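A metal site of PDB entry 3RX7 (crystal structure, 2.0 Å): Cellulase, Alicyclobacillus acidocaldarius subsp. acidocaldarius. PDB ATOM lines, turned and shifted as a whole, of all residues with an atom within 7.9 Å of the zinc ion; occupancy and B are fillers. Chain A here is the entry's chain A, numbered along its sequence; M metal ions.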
ATOM      1  N   GLN A 102      17.552  16.478 -27.427  1.00  0.00           N
ATOM      2  CA  GLN A 102      18.083  17.636 -26.670  1.00  0.00           C
ATOM      3  C   GLN A 102      19.368  17.294 -25.939  1.00  0.00           C
ATOM      4  O   GLN A 102      19.964  18.208 -25.372  1.00  0.00           O
ATOM      5  CB  GLN A 102      17.052  18.145 -25.626  1.00  0.00           C
ATOM      6  CG  GLN A 102      15.864  18.890 -26.211  1.00  0.00           C
ATOM      7  CD  GLN A 102      16.203  20.171 -26.940  1.00  0.00           C
ATOM      8  OE1 GLN A 102      16.480  20.153 -28.131  1.00  0.00           O
ATOM      9  NE2 GLN A 102      16.141  21.325 -26.269  1.00  0.00           N
ATOM     10  N   LEU A 103      19.790  15.998 -25.937  1.00  0.00           N
ATOM     11  CA  LEU A 103      20.997  15.585 -25.209  1.00  0.00           C
ATOM     12  C   LEU A 103      22.230  16.411 -25.540  1.00  0.00           C
ATOM     13  O   LEU A 103      22.503  16.686 -26.709  1.00  0.00           O
ATOM     14  CB  LEU A 103      21.321  14.089 -25.345  1.00  0.00           C
ATOM     15  CG  LEU A 103      20.457  13.101 -24.528  1.00  0.00           C
ATOM     16  CD1 LEU A 103      20.701  11.687 -24.986  1.00  0.00           C
ATOM     17  CD2 LEU A 103      20.703  13.259 -23.025  1.00  0.00           C
ATOM     18  N   CYS A 104      22.977  16.825 -24.493  1.00  0.00           N
ATOM     19  CA  CYS A 104      24.186  17.643 -24.635  1.00  0.00           C
ATOM     20  C   CYS A 104      25.407  16.787 -24.305  1.00  0.00           C
ATOM     21  O   CYS A 104      25.347  16.024 -23.349  1.00  0.00           O
ATOM     22  CB  CYS A 104      24.083  18.829 -23.675  1.00  0.00           C
ATOM     23  SG  CYS A 104      25.453  20.002 -23.792  1.00  0.00           S
ATOM     24  N   GLY A 105      26.504  16.969 -25.037  1.00  0.00           N
ATOM     25  CA  GLY A 105      27.771  16.274 -24.769  1.00  0.00           C
ATOM     26  C   GLY A 105      27.794  14.801 -25.140  1.00  0.00           C
ATOM     27  O   GLY A 105      28.656  14.050 -24.665  1.00  0.00           O
ATOM     28  N   VAL A 106      26.827  14.388 -25.969  1.00  0.00           N
ATOM     29  CA  VAL A 106      26.585  12.980 -26.335  1.00  0.00           C
ATOM     30  C   VAL A 106      26.506  12.863 -27.844  1.00  0.00           C
ATOM     31  O   VAL A 106      25.842  13.674 -28.503  1.00  0.00           O
ATOM     32  CB  VAL A 106      25.251  12.483 -25.676  1.00  0.00           C
ATOM     33  CG1 VAL A 106      24.995  11.002 -25.928  1.00  0.00           C
ATOM     34  CG2 VAL A 106      25.221  12.781 -24.178  1.00  0.00           C
ATOM     35  N   HIS A 118      24.110  14.433 -34.736  1.00  0.00           N
ATOM     36  CA  HIS A 118      25.232  15.339 -34.478  1.00  0.00           C
ATOM     37  C   HIS A 118      26.200  14.738 -33.484  1.00  0.00           C
ATOM     38  O   HIS A 118      25.830  13.818 -32.732  1.00  0.00           O
ATOM     39  CB  HIS A 118      24.768  16.756 -34.027  1.00  0.00           C
ATOM     40  CG  HIS A 118      24.134  16.844 -32.666  1.00  0.00           C
ATOM     41  ND1 HIS A 118      24.888  16.784 -31.507  1.00  0.00           N
ATOM     42  CD2 HIS A 118      22.828  17.050 -32.329  1.00  0.00           C
ATOM     43  CE1 HIS A 118      24.031  16.919 -30.502  1.00  0.00           C
ATOM     44  NE2 HIS A 118      22.781  17.092 -30.955  1.00  0.00           N
ATOM     45  N   GLY A 119      27.425  15.270 -33.480  1.00  0.00           N
ATOM     46  CA  GLY A 119      28.483  14.865 -32.569  1.00  0.00           C
ATOM     47  C   GLY A 119      28.320  15.542 -31.222  1.00  0.00           C
ATOM     48  O   GLY A 119      27.489  16.438 -31.074  1.00  0.00           O
ATOM     49  N   ALA A 120      29.115  15.114 -30.233  1.00  0.00           N
ATOM     50  CA  ALA A 120      29.086  15.634 -28.861  1.00  0.00           C
ATOM     51  C   ALA A 120      29.334  17.163 -28.804  1.00  0.00           C
ATOM     52  O   ALA A 120      30.298  17.668 -29.376  1.00  0.00           O
ATOM     53  CB  ALA A 120      30.096  14.902 -27.997  1.00  0.00           C
ATOM     54  N   CYS A 121      28.423  17.884 -28.147  1.00  0.00           N
ATOM     55  CA  CYS A 121      28.490  19.344 -28.045  1.00  0.00           C
ATOM     56  C   CYS A 121      28.812  19.789 -26.640  1.00  0.00           C
ATOM     57  O   CYS A 121      28.572  19.033 -25.694  1.00  0.00           O
ATOM     58  CB  CYS A 121      27.177  19.949 -28.519  1.00  0.00           C
ATOM     59  SG  CYS A 121      25.730  19.315 -27.631  1.00  0.00           S
ATOM     60  N   HIS A 122      29.331  21.026 -26.505  1.00  0.00           N
ATOM     61  CA  HIS A 122      29.611  21.667 -25.215  1.00  0.00           C
ATOM     62  C   HIS A 122      30.429  20.760 -24.315  1.00  0.00           C
ATOM     63  O   HIS A 122      30.046  20.556 -23.151  1.00  0.00           O
ATOM     64  CB  HIS A 122      28.282  22.074 -24.543  1.00  0.00           C
ATOM     65  CG  HIS A 122      27.450  22.948 -25.417  1.00  0.00           C
ATOM     66  ND1 HIS A 122      26.375  22.446 -26.108  1.00  0.00           N
ATOM     67  CD2 HIS A 122      27.591  24.258 -25.722  1.00  0.00           C
ATOM     68  CE1 HIS A 122      25.894  23.450 -26.816  1.00  0.00           C
ATOM     69  NE2 HIS A 122      26.598  24.571 -26.605  1.00  0.00           N
ATOM     70  N   THR A 123      31.498  20.154 -24.874  1.00  0.00           N
ATOM     71  CA  THR A 123      32.357  19.210 -24.164  1.00  0.00           C
ATOM     72  C   THR A 123      33.312  19.827 -23.156  1.00  0.00           C
ATOM     73  O   THR A 123      33.820  19.113 -22.284  1.00  0.00           O
ATOM     74  CB  THR A 123      32.981  18.157 -25.101  1.00  0.00           C
ATOM     75  OG1 THR A 123      33.449  18.775 -26.309  1.00  0.00           O
ATOM     76  CG2 THR A 123      32.007  17.018 -25.429  1.00  0.00           C
ATOM     77  N   GLY A 139      26.520  16.515 -20.183  1.00  0.00           N
ATOM     78  CA  GLY A 139      25.287  15.756 -20.209  1.00  0.00           C
ATOM     79  C   GLY A 139      24.054  16.586 -19.948  1.00  0.00           C
ATOM     80  O   GLY A 139      24.096  17.817 -19.956  1.00  0.00           O
ATOM     81  N   GLY A 140      22.963  15.889 -19.755  1.00  0.00           N
ATOM     82  CA  GLY A 140      21.687  16.535 -19.528  1.00  0.00           C
ATOM     83  C   GLY A 140      21.109  17.046 -20.822  1.00  0.00           C
ATOM     84  O   GLY A 140      21.496  16.600 -21.898  1.00  0.00           O
ATOM     85  N   TRP A 141      20.185  17.997 -20.719  1.00  0.00           N
ATOM     86  CA  TRP A 141      19.480  18.456 -21.900  1.00  0.00           C
ATOM     87  C   TRP A 141      19.690  19.917 -22.162  1.00  0.00           C
ATOM     88  O   TRP A 141      19.754  20.726 -21.225  1.00  0.00           O
ATOM     89  CB  TRP A 141      17.951  18.217 -21.721  1.00  0.00           C
ATOM     90  CG  TRP A 141      17.541  16.790 -21.447  1.00  0.00           C
ATOM     91  CD1 TRP A 141      18.048  15.659 -22.011  1.00  0.00           C
ATOM     92  CD2 TRP A 141      16.528  16.353 -20.508  1.00  0.00           C
ATOM     93  NE1 TRP A 141      17.412  14.543 -21.503  1.00  0.00           N
ATOM     94  CE2 TRP A 141      16.485  14.941 -20.575  1.00  0.00           C
ATOM     95  CE3 TRP A 141      15.688  17.019 -19.591  1.00  0.00           C
ATOM     96  CZ2 TRP A 141      15.581  14.185 -19.803  1.00  0.00           C
ATOM     97  CZ3 TRP A 141      14.780  16.270 -18.850  1.00  0.00           C
ATOM     98  CH2 TRP A 141      14.766  14.866 -18.936  1.00  0.00           C
ATOM     99  N   HIS A 142      19.682  20.269 -23.448  1.00  0.00           N
ATOM    100  CA  HIS A 142      19.604  21.656 -23.868  1.00  0.00           C
ATOM    101  C   HIS A 142      18.160  21.976 -23.452  1.00  0.00           C
ATOM    102  O   HIS A 142      17.251  21.156 -23.635  1.00  0.00           O
ATOM    103  CB  HIS A 142      19.770  21.809 -25.371  1.00  0.00           C
ATOM    104  CG  HIS A 142      21.105  21.397 -25.886  1.00  0.00           C
ATOM    105  ND1 HIS A 142      21.228  20.666 -27.058  1.00  0.00           N
ATOM    106  CD2 HIS A 142      22.338  21.605 -25.365  1.00  0.00           C
ATOM    107  CE1 HIS A 142      22.526  20.486 -27.231  1.00  0.00           C
ATOM    108  NE2 HIS A 142      23.240  21.024 -26.238  1.00  0.00           N
ATOM    109  N   ASP A 146      17.564  27.124 -27.160  1.00  0.00           N
ATOM    110  CA  ASP A 146      18.956  27.521 -26.872  1.00  0.00           C
ATOM    111  C   ASP A 146      19.699  26.311 -26.256  1.00  0.00           C
ATOM    112  O   ASP A 146      19.102  25.255 -26.060  1.00  0.00           O
ATOM    113  CB  ASP A 146      18.996  28.748 -25.939  1.00  0.00           C
ATOM    114  CG  ASP A 146      18.604  28.439 -24.508  1.00  0.00           C
ATOM    115  OD1 ASP A 146      17.508  27.864 -24.302  1.00  0.00           O
ATOM    116  OD2 ASP A 146      19.415  28.701 -23.599  1.00  0.00           O
ATOM    117  N   TYR A 147      20.996  26.482 -25.978  1.00  0.00           N
ATOM    118  CA  TYR A 147      21.847  25.422 -25.484  1.00  0.00           C
ATOM    119  C   TYR A 147      22.166  25.447 -24.006  1.00  0.00           C
ATOM    120  O   TYR A 147      22.881  24.579 -23.525  1.00  0.00           O
ATOM    121  CB  TYR A 147      23.113  25.296 -26.359  1.00  0.00           C
ATOM    122  CG  TYR A 147      22.808  25.021 -27.828  1.00  0.00           C
ATOM    123  CD1 TYR A 147      22.010  23.953 -28.209  1.00  0.00           C
ATOM    124  CD2 TYR A 147      23.403  25.780 -28.834  1.00  0.00           C
ATOM    125  CE1 TYR A 147      21.725  23.694 -29.550  1.00  0.00           C
ATOM    126  CE2 TYR A 147      23.136  25.528 -30.186  1.00  0.00           C
ATOM    127  CZ  TYR A 147      22.294  24.481 -30.543  1.00  0.00           C
ATOM    128  OH  TYR A 147      22.032  24.222 -31.862  1.00  0.00           O
ATOM    129  N   GLY A 148      21.594  26.400 -23.285  1.00  0.00           N
ATOM    130  CA  GLY A 148      21.789  26.472 -21.833  1.00  0.00           C
ATOM    131  C   GLY A 148      21.160  25.307 -21.093  1.00  0.00           C
ATOM    132  O   GLY A 148      20.213  24.682 -21.570  1.00  0.00           O
ATOM    133  N   LYS A 149      21.711  24.976 -19.918  1.00  0.00           N
ATOM    134  CA  LYS A 149      21.190  23.889 -19.082  1.00  0.00           C
ATOM    135  C   LYS A 149      20.882  24.517 -17.734  1.00  0.00           C
ATOM    136  O   LYS A 149      21.780  24.939 -17.016  1.00  0.00           O
ATOM    137  CB  LYS A 149      22.159  22.702 -18.982  1.00  0.00           C
ATOM    138  CG  LYS A 149      22.646  22.220 -20.363  1.00  0.00           C
ATOM    139  CD  LYS A 149      23.464  20.939 -20.360  1.00  0.00           C
ATOM    140  CE  LYS A 149      24.818  21.070 -19.706  1.00  0.00           C
ATOM    141  NZ  LYS A 149      25.707  19.918 -20.055  1.00  0.00           N
ATOM    142  N   PRO A 228      24.568  22.586 -32.752  1.00  0.00           N
ATOM    143  CA  PRO A 228      25.023  22.381 -31.361  1.00  0.00           C
ATOM    144  C   PRO A 228      26.538  22.262 -31.205  1.00  0.00           C
ATOM    145  O   PRO A 228      27.128  22.951 -30.384  1.00  0.00           O
ATOM    146  CB  PRO A 228      24.276  21.103 -30.921  1.00  0.00           C
ATOM    147  CG  PRO A 228      23.778  20.488 -32.188  1.00  0.00           C
ATOM    148  CD  PRO A 228      23.524  21.609 -33.123  1.00  0.00           C
ATOM    149  N   GLU A 229      27.177  21.448 -32.072  1.00  0.00           N
ATOM    150  CA  GLU A 229      28.623  21.232 -32.008  1.00  0.00           C
ATOM    151  C   GLU A 229      29.491  22.402 -32.514  1.00  0.00           C
ATOM    152  O   GLU A 229      30.686  22.378 -32.294  1.00  0.00           O
ATOM    153  CB  GLU A 229      29.038  19.839 -32.518  1.00  0.00           C
ATOM    154  CG  GLU A 229      28.874  19.635 -34.017  1.00  0.00           C
ATOM    155  CD  GLU A 229      27.533  19.129 -34.509  1.00  0.00           C
ATOM    156  OE1 GLU A 229      26.484  19.723 -34.156  1.00  0.00           O
ATOM    157  OE2 GLU A 229      27.534  18.167 -35.309  1.00  0.00           O
ATOM    158  N   ASP A 231      28.797  25.514 -31.384  1.00  0.00           N
ATOM    159  CA  ASP A 231      28.674  26.471 -30.287  1.00  0.00           C
ATOM    160  C   ASP A 231      29.880  26.349 -29.350  1.00  0.00           C
ATOM    161  O   ASP A 231      29.852  25.625 -28.356  1.00  0.00           O
ATOM    162  CB  ASP A 231      27.323  26.296 -29.562  1.00  0.00           C
ATOM    163  CG  ASP A 231      27.055  27.354 -28.522  1.00  0.00           C
ATOM    164  OD1 ASP A 231      27.618  28.480 -28.650  1.00  0.00           O
ATOM    165  OD2 ASP A 231      26.301  27.060 -27.574  1.00  0.00           O
ATOM    166  N   LEU A 235      31.801  28.099 -21.510  1.00  0.00           N
ATOM    167  CA  LEU A 235      30.661  27.784 -20.636  1.00  0.00           C
ATOM    168  C   LEU A 235      30.896  28.383 -19.264  1.00  0.00           C
ATOM    169  O   LEU A 235      32.005  28.303 -18.724  1.00  0.00           O
ATOM    170  CB  LEU A 235      30.478  26.256 -20.525  1.00  0.00           C
ATOM    171  CG  LEU A 235      30.018  25.507 -21.793  1.00  0.00           C
ATOM    172  CD1 LEU A 235      30.094  24.013 -21.592  1.00  0.00           C
ATOM    173  CD2 LEU A 235      28.582  25.881 -22.208  1.00  0.00           C
HETATM  174 ZN    ZN M   1      25.302  20.687 -25.913  1.00  0.00          ZN
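O of Cys 121 sits at hydrogen-bond distance from N of Gly 105 (3.0 Å).
SG of Cys 104 sits close to NZ of Lys 149 (3.7 Å).
The backbone NH (N) of His 142 sits at hydrogen-bond distance from the backbone carbonyl oxygen (O) of Gln 102.
A ring nitrogen (NE2) of His 122 lies within hydrogen-bond range of the side-chain carboxylate of Asp 231.
The backbone NH (N) of Cys 104 is in hydrogen-bond range of the backbone carbonyl oxygen (O) of Gly 140 (3.0 Å).
The backbone NH of Gly 139 lies close to the backbone carbonyl oxygen of Cys 104, 3.4 Å away.
The zinc ion is bound by a ring nitrogen (ND1) of His 122 (2.1 Å), a ring nitrogen (NE2) of His 142 (2.1 Å), the side-chain sulfur (SG) of Cys 104 (2.2 Å) and the side-chain sulfur (SG) of Cys 121 (2.2 Å).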
